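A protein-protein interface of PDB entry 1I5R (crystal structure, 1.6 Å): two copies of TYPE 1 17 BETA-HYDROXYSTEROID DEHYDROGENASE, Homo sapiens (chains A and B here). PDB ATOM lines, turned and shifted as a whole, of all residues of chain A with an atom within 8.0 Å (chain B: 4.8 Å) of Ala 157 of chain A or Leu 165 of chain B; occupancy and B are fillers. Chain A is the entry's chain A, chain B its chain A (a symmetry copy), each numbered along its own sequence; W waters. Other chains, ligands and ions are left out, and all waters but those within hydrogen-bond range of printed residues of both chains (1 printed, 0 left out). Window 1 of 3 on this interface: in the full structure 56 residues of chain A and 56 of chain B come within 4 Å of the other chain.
SG of Cys 156 of chain A sits close to O of Gly 144 of chain A (3.3 Å).
The backbone carbonyl oxygen (O) of Asn 152 of chain A sits close to the side-chain sulfur (SG) of Cys 156 of chain A, at 3.2 Å.
N of Leu 149 of chain A is in hydrogen-bond range of SG of Cys 156 of chain A (3.4 Å).
The backbone carbonyl oxygen (O) of Gly 164 of chain B sits at hydrogen-bond distance from the side-chain hydroxyl (OG) of Ser 168 of chain B (2.7 Å).
Of the printed residues of chain B, Leu 149 of chain A touches Ser 168.
Of the printed residues of chain B, Ala 157 of chain A touches Ala 161 and Leu 165.
Of the printed residues of chain B, Ala 161 of chain A touches Ala 161.
Of the printed residues of chain B, Gly 164 of chain A touches Phe 160.
Leu 165 of chain B touches just these residues of chain A: Asp 153 and Ala 157.
Of the printed residues of chain A, Ser 168 of chain B touches Gly 148, Leu 149, Pro 150, Asp 153 and Cys 156.
The nearest printed residue of chain B that does not touch Ala 157 of chain A is Gly 164 of chain B (4.1 Å).
The nearest residue of chain A that does not touch Leu 165 of chain B is Leu 99 of chain A (4.1 Å).
Printed residues of chain B that touch a printed residue of chain A: Val 119, Leu 122, Phe 160, Ala 161, Glu 163, Gly 164, Leu 165, Glu 167, Ser 168 and Leu 169.
Of the 27 printed residues of chain A, 13 touch a printed residue of chain B.
Hydrophobic or aromatic side chains of chain A within 4 Å of the printed part of chain B: Leu 99, Val 107, Pro 150, Ala 157, Phe 160 and Ala 161.
Among the printed residues, 23 pairs touch across the chains.
Among the printed residues, no Asp or Glu carboxylate lies within 4 Å of a Lys or Arg side-chain nitrogen of the other chain.
Water W1 lies within hydrogen-bond range of the side-chain carboxylate (OD1) of Asp 153 of chain A (2.5 Å), the backbone NH (N) of Phe 151 of chain A (2.9 Å) and the backbone carbonyl oxygen (O) of Ser 168 of chain B (3.0 Å).
The side-chain carboxylate (OE1) of Glu 167 of chain B is in hydrogen-bond range of the backbone NH (N) of Gly 148 of chain A.
OD1 of Asp 153 of chain A lies within hydrogen-bond range of N of Leu 169 of chain B (3.1 Å).
N of Leu 149 of chain A is in hydrogen-bond range of OG of Ser 168 of chain B.
The side-chain sulfur (SG) of Cys 156 of chain A lies close to the side-chain hydroxyl (OG) of Ser 168 of chain B (3.5 Å).
Leu 99 of chain A touches Val 119 of chain B.
CD2 of Leu 99 of chain A touches CB of Leu 122 of chain B, at 3.4 Å.
CD2 of Leu 99 of chain A touches CD1 of Leu 169 of chain B, 3.9 Å away.
Ser 168 of chain B touches Gly 148 of chain A.
Ser 168 of chain B touches Pro 150 of chain A.
Ser 168 of chain B touches Asp 153 of chain A.
CA of Ala 161 of chain B touches O of Ala 157 of chain A, 3.1 Å away.
CB of Phe 160 of chain A touches O of Phe 160 of chain B, at 3.1 Å.
Phe 160 of chain A touches Gly 164 of chain B.
Gly 164 of chain A touches Phe 160 of chain B (N to CD2, 3.2 Å).
Phe 160 of chain B touches its own counterpart, Phe 160 of chain A.
Phe 160 of chain A touches Glu 163 of chain B, and with the chains exchanged Glu 163 of chain A touches Phe 160 of chain B.
Phe 160 of chain A touches Gly 164 of chain B, and with the chains exchanged Gly 164 of chain A touches Phe 160 of chain B.
Ala 161 of chain B touches its own counterpart, Ala 161 of chain A.
Of the 23 pairs that touch across the chains among the printed residues, 6 have their exchanged pair printed and touching as well.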
ATOM      1  N   LEU A  99     -22.484   9.135   5.322  1.00  0.00           N
ATOM      2  CA  LEU A  99     -23.299   7.994   5.744  1.00  0.00           C
ATOM      3  C   LEU A  99     -24.327   8.339   6.799  1.00  0.00           C
ATOM      4  O   LEU A  99     -25.512   8.012   6.704  1.00  0.00           O
ATOM      5  CB  LEU A  99     -22.381   6.890   6.279  1.00  0.00           C
ATOM      6  CG  LEU A  99     -23.136   5.580   6.548  1.00  0.00           C
ATOM      7  CD1 LEU A  99     -23.489   4.945   5.207  1.00  0.00           C
ATOM      8  CD2 LEU A  99     -22.308   4.642   7.401  1.00  0.00           C
ATOM      9  N   LEU A 102     -27.545   9.966   5.670  1.00  0.00           N
ATOM     10  CA  LEU A 102     -28.461   9.223   4.814  1.00  0.00           C
ATOM     11  C   LEU A 102     -29.611   8.661   5.632  1.00  0.00           C
ATOM     12  O   LEU A 102     -29.384   8.091   6.696  1.00  0.00           O
ATOM     13  CB  LEU A 102     -27.738   8.063   4.129  1.00  0.00           C
ATOM     14  CG  LEU A 102     -26.441   8.444   3.417  1.00  0.00           C
ATOM     15  CD1 LEU A 102     -25.830   7.187   2.814  1.00  0.00           C
ATOM     16  CD2 LEU A 102     -26.681   9.514   2.366  1.00  0.00           C
ATOM     17  N   VAL A 107     -31.220   4.395   2.543  1.00  0.00           N
ATOM     18  CA  VAL A 107     -30.211   3.338   2.474  1.00  0.00           C
ATOM     19  C   VAL A 107     -30.850   2.022   2.076  1.00  0.00           C
ATOM     20  O   VAL A 107     -30.382   1.314   1.189  1.00  0.00           O
ATOM     21  CB  VAL A 107     -29.519   3.165   3.835  1.00  0.00           C
ATOM     22  CG1 VAL A 107     -28.610   1.944   3.850  1.00  0.00           C
ATOM     23  CG2 VAL A 107     -28.738   4.437   4.106  1.00  0.00           C
ATOM     24  N   VAL A 110     -31.895   1.844  -1.542  1.00  0.00           N
ATOM     25  CA  VAL A 110     -30.804   1.665  -2.498  1.00  0.00           C
ATOM     26  C   VAL A 110     -30.478   0.176  -2.586  1.00  0.00           C
ATOM     27  O   VAL A 110     -30.337  -0.336  -3.690  1.00  0.00           O
ATOM     28  CB  VAL A 110     -29.555   2.442  -2.071  1.00  0.00           C
ATOM     29  CG1 VAL A 110     -28.332   2.049  -2.881  1.00  0.00           C
ATOM     30  CG2 VAL A 110     -29.845   3.926  -2.205  1.00  0.00           C
ATOM     31  N   LEU A 111     -30.395  -0.479  -1.427  1.00  0.00           N
ATOM     32  CA  LEU A 111     -30.096  -1.905  -1.478  1.00  0.00           C
ATOM     33  C   LEU A 111     -31.260  -2.669  -2.095  1.00  0.00           C
ATOM     34  O   LEU A 111     -31.064  -3.588  -2.869  1.00  0.00           O
ATOM     35  CB  LEU A 111     -29.794  -2.433  -0.080  1.00  0.00           C
ATOM     36  CG  LEU A 111     -28.384  -2.233   0.463  1.00  0.00           C
ATOM     37  CD1 LEU A 111     -27.357  -2.848  -0.489  1.00  0.00           C
ATOM     38  CD2 LEU A 111     -28.048  -0.779   0.701  1.00  0.00           C
ATOM     39  N   ASN A 114     -31.250  -1.642  -5.967  1.00  0.00           N
ATOM     40  CA  ASN A 114     -30.051  -2.028  -6.703  1.00  0.00           C
ATOM     41  C   ASN A 114     -29.718  -3.505  -6.585  1.00  0.00           C
ATOM     42  O   ASN A 114     -29.307  -4.122  -7.565  1.00  0.00           O
ATOM     43  CB  ASN A 114     -28.838  -1.221  -6.218  1.00  0.00           C
ATOM     44  CG  ASN A 114     -29.062   0.252  -6.530  1.00  0.00           C
ATOM     45  OD1 ASN A 114     -30.112   0.649  -7.024  1.00  0.00           O
ATOM     46  ND2 ASN A 114     -28.069   1.074  -6.221  1.00  0.00           N
ATOM     47  N   VAL A 115     -29.857  -3.985  -5.364  1.00  0.00           N
ATOM     48  CA  VAL A 115     -29.480  -5.388  -5.142  1.00  0.00           C
ATOM     49  C   VAL A 115     -30.683  -6.303  -5.133  1.00  0.00           C
ATOM     50  O   VAL A 115     -30.754  -7.160  -5.993  1.00  0.00           O
ATOM     51  CB  VAL A 115     -28.689  -5.516  -3.835  1.00  0.00           C
ATOM     52  CG1 VAL A 115     -28.078  -6.903  -3.722  1.00  0.00           C
ATOM     53  CG2 VAL A 115     -27.608  -4.447  -3.811  1.00  0.00           C
ATOM     54  N   GLY A 144     -17.912   2.211  -9.220  1.00  0.00           N
ATOM     55  CA  GLY A 144     -18.170   2.326  -7.795  1.00  0.00           C
ATOM     56  C   GLY A 144     -18.569   0.987  -7.173  1.00  0.00           C
ATOM     57  O   GLY A 144     -18.751   0.879  -5.969  1.00  0.00           O
ATOM     58  N   GLY A 145     -18.745  -0.044  -7.989  1.00  0.00           N
ATOM     59  CA  GLY A 145     -19.000  -1.388  -7.526  1.00  0.00           C
ATOM     60  C   GLY A 145     -17.672  -2.143  -7.430  1.00  0.00           C
ATOM     61  O   GLY A 145     -17.619  -3.255  -6.921  1.00  0.00           O
ATOM     62  N   MET A 147     -14.696  -0.195  -6.593  1.00  0.00           N
ATOM     63  CA  MET A 147     -13.823   0.535  -5.679  1.00  0.00           C
ATOM     64  C   MET A 147     -14.694   1.524  -4.925  1.00  0.00           C
ATOM     65  O   MET A 147     -15.677   2.003  -5.482  1.00  0.00           O
ATOM     66  CB  MET A 147     -12.737   1.213  -6.487  1.00  0.00           C
ATOM     67  CG  MET A 147     -13.325   2.303  -7.379  1.00  0.00           C
ATOM     68  SD  MET A 147     -12.004   2.905  -8.434  1.00  0.00           S
ATOM     69  CE  MET A 147     -12.603   4.560  -8.773  1.00  0.00           C
ATOM     70  N   GLY A 148     -14.366   1.700  -3.662  1.00  0.00           N
ATOM     71  CA  GLY A 148     -15.194   2.516  -2.789  1.00  0.00           C
ATOM     72  C   GLY A 148     -14.942   3.988  -3.052  1.00  0.00           C
ATOM     73  O   GLY A 148     -13.840   4.413  -3.333  1.00  0.00           O
ATOM     74  N   LEU A 149     -16.032   4.723  -2.953  1.00  0.00           N
ATOM     75  CA  LEU A 149     -15.983   6.173  -3.174  1.00  0.00           C
ATOM     76  C   LEU A 149     -16.576   6.815  -1.935  1.00  0.00           C
ATOM     77  O   LEU A 149     -17.662   6.457  -1.508  1.00  0.00           O
ATOM     78  CB  LEU A 149     -16.775   6.518  -4.413  1.00  0.00           C
ATOM     79  CG  LEU A 149     -16.090   6.079  -5.719  1.00  0.00           C
ATOM     80  CD1 LEU A 149     -17.015   6.392  -6.880  1.00  0.00           C
ATOM     81  CD2 LEU A 149     -14.744   6.769  -5.880  1.00  0.00           C
ATOM     82  N   PRO A 150     -15.843   7.764  -1.385  1.00  0.00           N
ATOM     83  CA  PRO A 150     -16.313   8.440  -0.188  1.00  0.00           C
ATOM     84  C   PRO A 150     -17.627   9.086  -0.541  1.00  0.00           C
ATOM     85  O   PRO A 150     -17.875   9.519  -1.663  1.00  0.00           O
ATOM     86  CB  PRO A 150     -15.204   9.421   0.144  1.00  0.00           C
ATOM     87  CG  PRO A 150     -14.551   9.680  -1.181  1.00  0.00           C
ATOM     88  CD  PRO A 150     -14.586   8.348  -1.905  1.00  0.00           C
ATOM     89  N   PHE A 151     -18.533   9.099   0.425  1.00  0.00           N
ATOM     90  CA  PHE A 151     -19.851   9.667   0.317  1.00  0.00           C
ATOM     91  C   PHE A 151     -20.787   8.898  -0.596  1.00  0.00           C
ATOM     92  O   PHE A 151     -21.929   9.258  -0.760  1.00  0.00           O
ATOM     93  CB  PHE A 151     -19.818  11.139  -0.103  1.00  0.00           C
ATOM     94  CG  PHE A 151     -19.045  11.941   0.915  1.00  0.00           C
ATOM     95  CD1 PHE A 151     -19.595  12.182   2.160  1.00  0.00           C
ATOM     96  CD2 PHE A 151     -17.771  12.393   0.622  1.00  0.00           C
ATOM     97  CE1 PHE A 151     -18.893  12.901   3.106  1.00  0.00           C
ATOM     98  CE2 PHE A 151     -17.052  13.072   1.582  1.00  0.00           C
ATOM     99  CZ  PHE A 151     -17.617  13.332   2.815  1.00  0.00           C
ATOM    100  N   ASN A 152     -20.320   7.756  -1.078  1.00  0.00           N
ATOM    101  CA  ASN A 152     -21.124   6.872  -1.908  1.00  0.00           C
ATOM    102  C   ASN A 152     -21.095   5.503  -1.239  1.00  0.00           C
ATOM    103  O   ASN A 152     -21.252   4.491  -1.909  1.00  0.00           O
ATOM    104  CB  ASN A 152     -20.455   6.702  -3.270  1.00  0.00           C
ATOM    105  CG  ASN A 152     -20.651   7.966  -4.082  1.00  0.00           C
ATOM    106  OD1 ASN A 152     -21.623   8.066  -4.825  1.00  0.00           O
ATOM    107  ND2 ASN A 152     -19.730   8.885  -3.873  1.00  0.00           N
ATOM    108  N   ASP A 153     -20.948   5.510   0.075  1.00  0.00           N
ATOM    109  CA  ASP A 153     -20.813   4.281   0.836  1.00  0.00           C
ATOM    110  C   ASP A 153     -21.904   3.281   0.509  1.00  0.00           C
ATOM    111  O   ASP A 153     -21.616   2.109   0.265  1.00  0.00           O
ATOM    112  CB  ASP A 153     -20.921   4.555   2.344  1.00  0.00           C
ATOM    113  CG  ASP A 153     -20.056   5.748   2.719  1.00  0.00           C
ATOM    114  OD1 ASP A 153     -18.850   5.687   2.494  1.00  0.00           O
ATOM    115  OD2 ASP A 153     -20.641   6.698   3.257  1.00  0.00           O
ATOM    116  N   VAL A 154     -23.133   3.773   0.508  1.00  0.00           N
ATOM    117  CA  VAL A 154     -24.242   2.847   0.276  1.00  0.00           C
ATOM    118  C   VAL A 154     -24.389   2.523  -1.186  1.00  0.00           C
ATOM    119  O   VAL A 154     -24.694   1.402  -1.569  1.00  0.00           O
ATOM    120  CB  VAL A 154     -25.529   3.409   0.884  1.00  0.00           C
ATOM    121  CG1 VAL A 154     -26.721   2.534   0.534  1.00  0.00           C
ATOM    122  CG2 VAL A 154     -25.309   3.515   2.386  1.00  0.00           C
ATOM    123  N   TYR A 155     -24.178   3.557  -2.011  1.00  0.00           N
ATOM    124  CA  TYR A 155     -24.248   3.331  -3.450  1.00  0.00           C
ATOM    125  C   TYR A 155     -23.217   2.275  -3.819  1.00  0.00           C
ATOM    126  O   TYR A 155     -23.527   1.289  -4.463  1.00  0.00           O
ATOM    127  CB  TYR A 155     -23.972   4.646  -4.176  1.00  0.00           C
ATOM    128  CG  TYR A 155     -23.850   4.381  -5.664  1.00  0.00           C
ATOM    129  CD1 TYR A 155     -24.971   4.143  -6.440  1.00  0.00           C
ATOM    130  CD2 TYR A 155     -22.588   4.379  -6.235  1.00  0.00           C
ATOM    131  CE1 TYR A 155     -24.822   3.909  -7.800  1.00  0.00           C
ATOM    132  CE2 TYR A 155     -22.442   4.128  -7.583  1.00  0.00           C
ATOM    133  CZ  TYR A 155     -23.565   3.907  -8.349  1.00  0.00           C
ATOM    134  OH  TYR A 155     -23.351   3.654  -9.687  1.00  0.00           O
ATOM    135  N   CYS A 156     -21.976   2.512  -3.353  1.00  0.00           N
ATOM    136  CA  CYS A 156     -20.923   1.543  -3.653  1.00  0.00           C
ATOM    137  C   CYS A 156     -21.255   0.193  -3.041  1.00  0.00           C
ATOM    138  O   CYS A 156     -21.083  -0.828  -3.669  1.00  0.00           O
ATOM    139  CB  CYS A 156     -19.598   2.013  -3.059  1.00  0.00           C
ATOM    140  SG  CYS A 156     -19.010   3.459  -3.994  1.00  0.00           S
ATOM    141  N   ALA A 157     -21.765   0.236  -1.806  1.00  0.00           N
ATOM    142  CA  ALA A 157     -22.135  -1.049  -1.190  1.00  0.00           C
ATOM    143  C   ALA A 157     -23.063  -1.798  -2.146  1.00  0.00           C
ATOM    144  O   ALA A 157     -22.886  -2.974  -2.423  1.00  0.00           O
ATOM    145  CB  ALA A 157     -22.850  -0.798   0.122  1.00  0.00           C
ATOM    146  N   SER A 158     -24.055  -1.080  -2.689  1.00  0.00           N
ATOM    147  CA  SER A 158     -25.004  -1.735  -3.583  1.00  0.00           C
ATOM    148  C   SER A 158     -24.377  -2.211  -4.872  1.00  0.00           C
ATOM    149  O   SER A 158     -24.770  -3.241  -5.410  1.00  0.00           O
ATOM    150  CB  SER A 158     -26.174  -0.795  -3.878  1.00  0.00           C
ATOM    151  OG  SER A 158     -25.819   0.185  -4.825  1.00  0.00           O
ATOM    152  N   LYS A 159     -23.431  -1.435  -5.410  1.00  0.00           N
ATOM    153  CA  LYS A 159     -22.825  -1.802  -6.688  1.00  0.00           C
ATOM    154  C   LYS A 159     -21.843  -2.936  -6.462  1.00  0.00           C
ATOM    155  O   LYS A 159     -21.695  -3.814  -7.290  1.00  0.00           O
ATOM    156  CB  LYS A 159     -22.136  -0.596  -7.319  1.00  0.00           C
ATOM    157  CG  LYS A 159     -23.106   0.538  -7.608  1.00  0.00           C
ATOM    158  CD  LYS A 159     -24.298   0.113  -8.425  1.00  0.00           C
ATOM    159  CE  LYS A 159     -23.955  -0.466  -9.778  1.00  0.00           C
ATOM    160  NZ  LYS A 159     -25.095  -0.346 -10.747  1.00  0.00           N
ATOM    161  N   PHE A 160     -21.171  -2.883  -5.304  1.00  0.00           N
ATOM    162  CA  PHE A 160     -20.261  -3.974  -4.958  1.00  0.00           C
ATOM    163  C   PHE A 160     -21.128  -5.219  -4.771  1.00  0.00           C
ATOM    164  O   PHE A 160     -20.742  -6.298  -5.192  1.00  0.00           O
ATOM    165  CB  PHE A 160     -19.613  -3.745  -3.599  1.00  0.00           C
ATOM    166  CG  PHE A 160     -18.315  -3.023  -3.657  1.00  0.00           C
ATOM    167  CD1 PHE A 160     -18.251  -1.730  -4.114  1.00  0.00           C
ATOM    168  CD2 PHE A 160     -17.146  -3.627  -3.228  1.00  0.00           C
ATOM    169  CE1 PHE A 160     -17.055  -1.049  -4.145  1.00  0.00           C
ATOM    170  CE2 PHE A 160     -15.942  -2.950  -3.257  1.00  0.00           C
ATOM    171  CZ  PHE A 160     -15.902  -1.664  -3.724  1.00  0.00           C
ATOM    172  N   ALA A 161     -22.274  -5.032  -4.127  1.00  0.00           N
ATOM    173  CA  ALA A 161     -23.202  -6.153  -3.929  1.00  0.00           C
ATOM    174  C   ALA A 161     -23.557  -6.780  -5.267  1.00  0.00           C
ATOM    175  O   ALA A 161     -23.520  -8.004  -5.399  1.00  0.00           O
ATOM    176  CB  ALA A 161     -24.446  -5.695  -3.203  1.00  0.00           C
ATOM    177  N   LEU A 162     -23.791  -5.948  -6.289  1.00  0.00           N
ATOM    178  CA  LEU A 162     -24.084  -6.502  -7.602  1.00  0.00           C
ATOM    179  C   LEU A 162     -22.924  -7.312  -8.140  1.00  0.00           C
ATOM    180  O   LEU A 162     -23.120  -8.308  -8.803  1.00  0.00           O
ATOM    181  CB  LEU A 162     -24.394  -5.374  -8.592  1.00  0.00           C
ATOM    182  CG  LEU A 162     -25.751  -4.719  -8.368  1.00  0.00           C
ATOM    183  CD1 LEU A 162     -25.924  -3.575  -9.353  1.00  0.00           C
ATOM    184  CD2 LEU A 162     -26.846  -5.762  -8.567  1.00  0.00           C
ATOM    185  N   GLU A 163     -21.692  -6.858  -7.879  1.00  0.00           N
ATOM    186  CA  GLU A 163     -20.533  -7.618  -8.296  1.00  0.00           C
ATOM    187  C   GLU A 163     -20.591  -9.002  -7.655  1.00  0.00           C
ATOM    188  O   GLU A 163     -20.418  -9.997  -8.327  1.00  0.00           O
ATOM    189  CB  GLU A 163     -19.234  -6.950  -7.818  1.00  0.00           C
ATOM    190  CG  GLU A 163     -19.123  -5.559  -8.452  1.00  0.00           C
ATOM    191  CD  GLU A 163     -18.814  -5.721  -9.929  1.00  0.00           C
ATOM    192  OE1 GLU A 163     -18.004  -6.585 -10.297  1.00  0.00           O
ATOM    193  OE2 GLU A 163     -19.413  -4.962 -10.705  1.00  0.00           O
ATOM    194  N   GLY A 164     -20.816  -9.032  -6.334  1.00  0.00           N
ATOM    195  CA  GLY A 164     -20.811 -10.317  -5.642  1.00  0.00           C
ATOM    196  C   GLY A 164     -21.973 -11.166  -6.146  1.00  0.00           C
ATOM    197  O   GLY A 164     -21.816 -12.347  -6.417  1.00  0.00           O
ATOM    198  N   VAL B 115     -25.834  -5.587   5.485  1.00  0.00           N
ATOM    199  CA  VAL B 115     -25.431  -4.275   4.960  1.00  0.00           C
ATOM    200  C   VAL B 115     -26.118  -3.140   5.685  1.00  0.00           C
ATOM    201  O   VAL B 115     -25.424  -2.355   6.303  1.00  0.00           O
ATOM    202  CB  VAL B 115     -25.708  -4.206   3.453  1.00  0.00           C
ATOM    203  CG1 VAL B 115     -25.068  -2.965   2.855  1.00  0.00           C
ATOM    204  CG2 VAL B 115     -25.162  -5.465   2.798  1.00  0.00           C
ATOM    205  N   THR B 118     -25.198  -2.904   9.298  1.00  0.00           N
ATOM    206  CA  THR B 118     -23.878  -2.323   9.505  1.00  0.00           C
ATOM    207  C   THR B 118     -23.944  -0.828   9.288  1.00  0.00           C
ATOM    208  O   THR B 118     -23.387  -0.058  10.064  1.00  0.00           O
ATOM    209  CB  THR B 118     -22.914  -2.970   8.501  1.00  0.00           C
ATOM    210  OG1 THR B 118     -23.001  -4.368   8.817  1.00  0.00           O
ATOM    211  CG2 THR B 118     -21.528  -2.412   8.698  1.00  0.00           C
ATOM    212  N   VAL B 119     -24.675  -0.431   8.238  1.00  0.00           N
ATOM    213  CA  VAL B 119     -24.870   1.017   8.055  1.00  0.00           C
ATOM    214  C   VAL B 119     -25.492   1.621   9.301  1.00  0.00           C
ATOM    215  O   VAL B 119     -25.029   2.639   9.804  1.00  0.00           O
ATOM    216  CB  VAL B 119     -25.785   1.301   6.856  1.00  0.00           C
ATOM    217  CG1 VAL B 119     -26.188   2.768   6.848  1.00  0.00           C
ATOM    218  CG2 VAL B 119     -24.991   0.921   5.610  1.00  0.00           C
ATOM    219  N   LEU B 122     -22.952   2.016  11.908  1.00  0.00           N
ATOM    220  CA  LEU B 122     -22.030   3.103  11.601  1.00  0.00           C
ATOM    221  C   LEU B 122     -22.707   4.442  11.759  1.00  0.00           C
ATOM    222  O   LEU B 122     -22.123   5.387  12.289  1.00  0.00           O
ATOM    223  CB  LEU B 122     -21.508   2.912  10.176  1.00  0.00           C
ATOM    224  CG  LEU B 122     -20.671   1.632  10.026  1.00  0.00           C
ATOM    225  CD1 LEU B 122     -20.465   1.295   8.559  1.00  0.00           C
ATOM    226  CD2 LEU B 122     -19.330   1.831  10.724  1.00  0.00           C
ATOM    227  N   PHE B 160     -19.857  -8.394  -0.264  1.00  0.00           N
ATOM    228  CA  PHE B 160     -19.216  -7.483  -1.213  1.00  0.00           C
ATOM    229  C   PHE B 160     -19.714  -6.079  -0.869  1.00  0.00           C
ATOM    230  O   PHE B 160     -18.940  -5.135  -0.898  1.00  0.00           O
ATOM    231  CB  PHE B 160     -19.702  -7.732  -2.634  1.00  0.00           C
ATOM    232  CG  PHE B 160     -18.875  -8.700  -3.400  1.00  0.00           C
ATOM    233  CD1 PHE B 160     -18.783 -10.012  -3.004  1.00  0.00           C
ATOM    234  CD2 PHE B 160     -18.202  -8.310  -4.544  1.00  0.00           C
ATOM    235  CE1 PHE B 160     -18.040 -10.918  -3.726  1.00  0.00           C
ATOM    236  CE2 PHE B 160     -17.453  -9.214  -5.273  1.00  0.00           C
ATOM    237  CZ  PHE B 160     -17.370 -10.515  -4.854  1.00  0.00           C
ATOM    238  N   ALA B 161     -21.004  -5.984  -0.569  1.00  0.00           N
ATOM    239  CA  ALA B 161     -21.578  -4.688  -0.184  1.00  0.00           C
ATOM    240  C   ALA B 161     -20.817  -4.108   0.996  1.00  0.00           C
ATOM    241  O   ALA B 161     -20.457  -2.930   0.974  1.00  0.00           O
ATOM    242  CB  ALA B 161     -23.047  -4.830   0.144  1.00  0.00           C
ATOM    243  N   LEU B 162     -20.468  -4.953   1.975  1.00  0.00           N
ATOM    244  CA  LEU B 162     -19.693  -4.455   3.100  1.00  0.00           C
ATOM    245  C   LEU B 162     -18.340  -3.937   2.663  1.00  0.00           C
ATOM    246  O   LEU B 162     -17.840  -2.977   3.208  1.00  0.00           O
ATOM    247  CB  LEU B 162     -19.481  -5.572   4.128  1.00  0.00           C
ATOM    248  CG  LEU B 162     -20.736  -5.923   4.918  1.00  0.00           C
ATOM    249  CD1 LEU B 162     -20.432  -7.083   5.852  1.00  0.00           C
ATOM    250  CD2 LEU B 162     -21.181  -4.701   5.715  1.00  0.00           C
ATOM    251  N   GLU B 163     -17.720  -4.607   1.683  1.00  0.00           N
ATOM    252  CA  GLU B 163     -16.458  -4.128   1.161  1.00  0.00           C
ATOM    253  C   GLU B 163     -16.650  -2.715   0.617  1.00  0.00           C
ATOM    254  O   GLU B 163     -15.879  -1.830   0.923  1.00  0.00           O
ATOM    255  CB  GLU B 163     -15.977  -5.003  -0.008  1.00  0.00           C
ATOM    256  CG  GLU B 163     -15.752  -6.433   0.497  1.00  0.00           C
ATOM    257  CD  GLU B 163     -14.513  -6.451   1.373  1.00  0.00           C
ATOM    258  OE1 GLU B 163     -13.514  -5.798   1.039  1.00  0.00           O
ATOM    259  OE2 GLU B 163     -14.578  -7.133   2.406  1.00  0.00           O
ATOM    260  N   GLY B 164     -17.687  -2.539  -0.214  1.00  0.00           N
ATOM    261  CA  GLY B 164     -17.887  -1.230  -0.830  1.00  0.00           C
ATOM    262  C   GLY B 164     -18.217  -0.209   0.252  1.00  0.00           C
ATOM    263  O   GLY B 164     -17.687   0.893   0.257  1.00  0.00           O
ATOM    264  N   LEU B 165     -19.064  -0.625   1.182  1.00  0.00           N
ATOM    265  CA  LEU B 165     -19.430   0.274   2.262  1.00  0.00           C
ATOM    266  C   LEU B 165     -18.214   0.738   3.052  1.00  0.00           C
ATOM    267  O   LEU B 165     -17.999   1.920   3.238  1.00  0.00           O
ATOM    268  CB  LEU B 165     -20.360  -0.467   3.221  1.00  0.00           C
ATOM    269  CG  LEU B 165     -20.790   0.356   4.442  1.00  0.00           C
ATOM    270  CD1 LEU B 165     -21.606   1.553   3.987  1.00  0.00           C
ATOM    271  CD2 LEU B 165     -21.582  -0.521   5.396  1.00  0.00           C
ATOM    272  N   CYS B 166     -17.439  -0.239   3.505  1.00  0.00           N
ATOM    273  CA  CYS B 166     -16.294   0.087   4.350  1.00  0.00           C
ATOM    274  C   CYS B 166     -15.185   0.789   3.612  1.00  0.00           C
ATOM    275  O   CYS B 166     -14.563   1.681   4.164  1.00  0.00           O
ATOM    276  CB  CYS B 166     -15.741  -1.211   4.958  1.00  0.00           C
ATOM    277  SG  CYS B 166     -16.943  -1.848   6.147  1.00  0.00           S
ATOM    278  N   GLU B 167     -14.961   0.361   2.367  1.00  0.00           N
ATOM    279  CA  GLU B 167     -13.893   1.004   1.612  1.00  0.00           C
ATOM    280  C   GLU B 167     -14.224   2.466   1.360  1.00  0.00           C
ATOM    281  O   GLU B 167     -13.380   3.331   1.514  1.00  0.00           O
ATOM    282  CB  GLU B 167     -13.735   0.252   0.303  1.00  0.00           C
ATOM    283  CG  GLU B 167     -12.494   0.746  -0.440  1.00  0.00           C
ATOM    284  CD  GLU B 167     -12.170  -0.294  -1.500  1.00  0.00           C
ATOM    285  OE1 GLU B 167     -12.499  -0.069  -2.675  1.00  0.00           O
ATOM    286  OE2 GLU B 167     -11.622  -1.329  -1.091  1.00  0.00           O
ATOM    287  N   SER B 168     -15.475   2.712   0.991  1.00  0.00           N
ATOM    288  CA  SER B 168     -15.959   4.062   0.762  1.00  0.00           C
ATOM    289  C   SER B 168     -15.805   4.895   2.025  1.00  0.00           C
ATOM    290  O   SER B 168     -15.302   6.012   1.964  1.00  0.00           O
ATOM    291  CB  SER B 168     -17.452   4.007   0.404  1.00  0.00           C
ATOM    292  OG  SER B 168     -17.537   3.324  -0.830  1.00  0.00           O
ATOM    293  N   LEU B 169     -16.192   4.292   3.150  1.00  0.00           N
ATOM    294  CA  LEU B 169     -16.055   5.021   4.405  1.00  0.00           C
ATOM    295  C   LEU B 169     -14.596   5.255   4.746  1.00  0.00           C
ATOM    296  O   LEU B 169     -14.214   6.342   5.169  1.00  0.00           O
ATOM    297  CB  LEU B 169     -16.704   4.206   5.524  1.00  0.00           C
ATOM    298  CG  LEU B 169     -18.227   4.357   5.515  1.00  0.00           C
ATOM    299  CD1 LEU B 169     -18.813   3.294   6.431  1.00  0.00           C
ATOM    300  CD2 LEU B 169     -18.606   5.754   5.980  1.00  0.00           C
HETATM  301  O   HOH W   1     -17.520   7.835   2.774  1.00  0.00           O
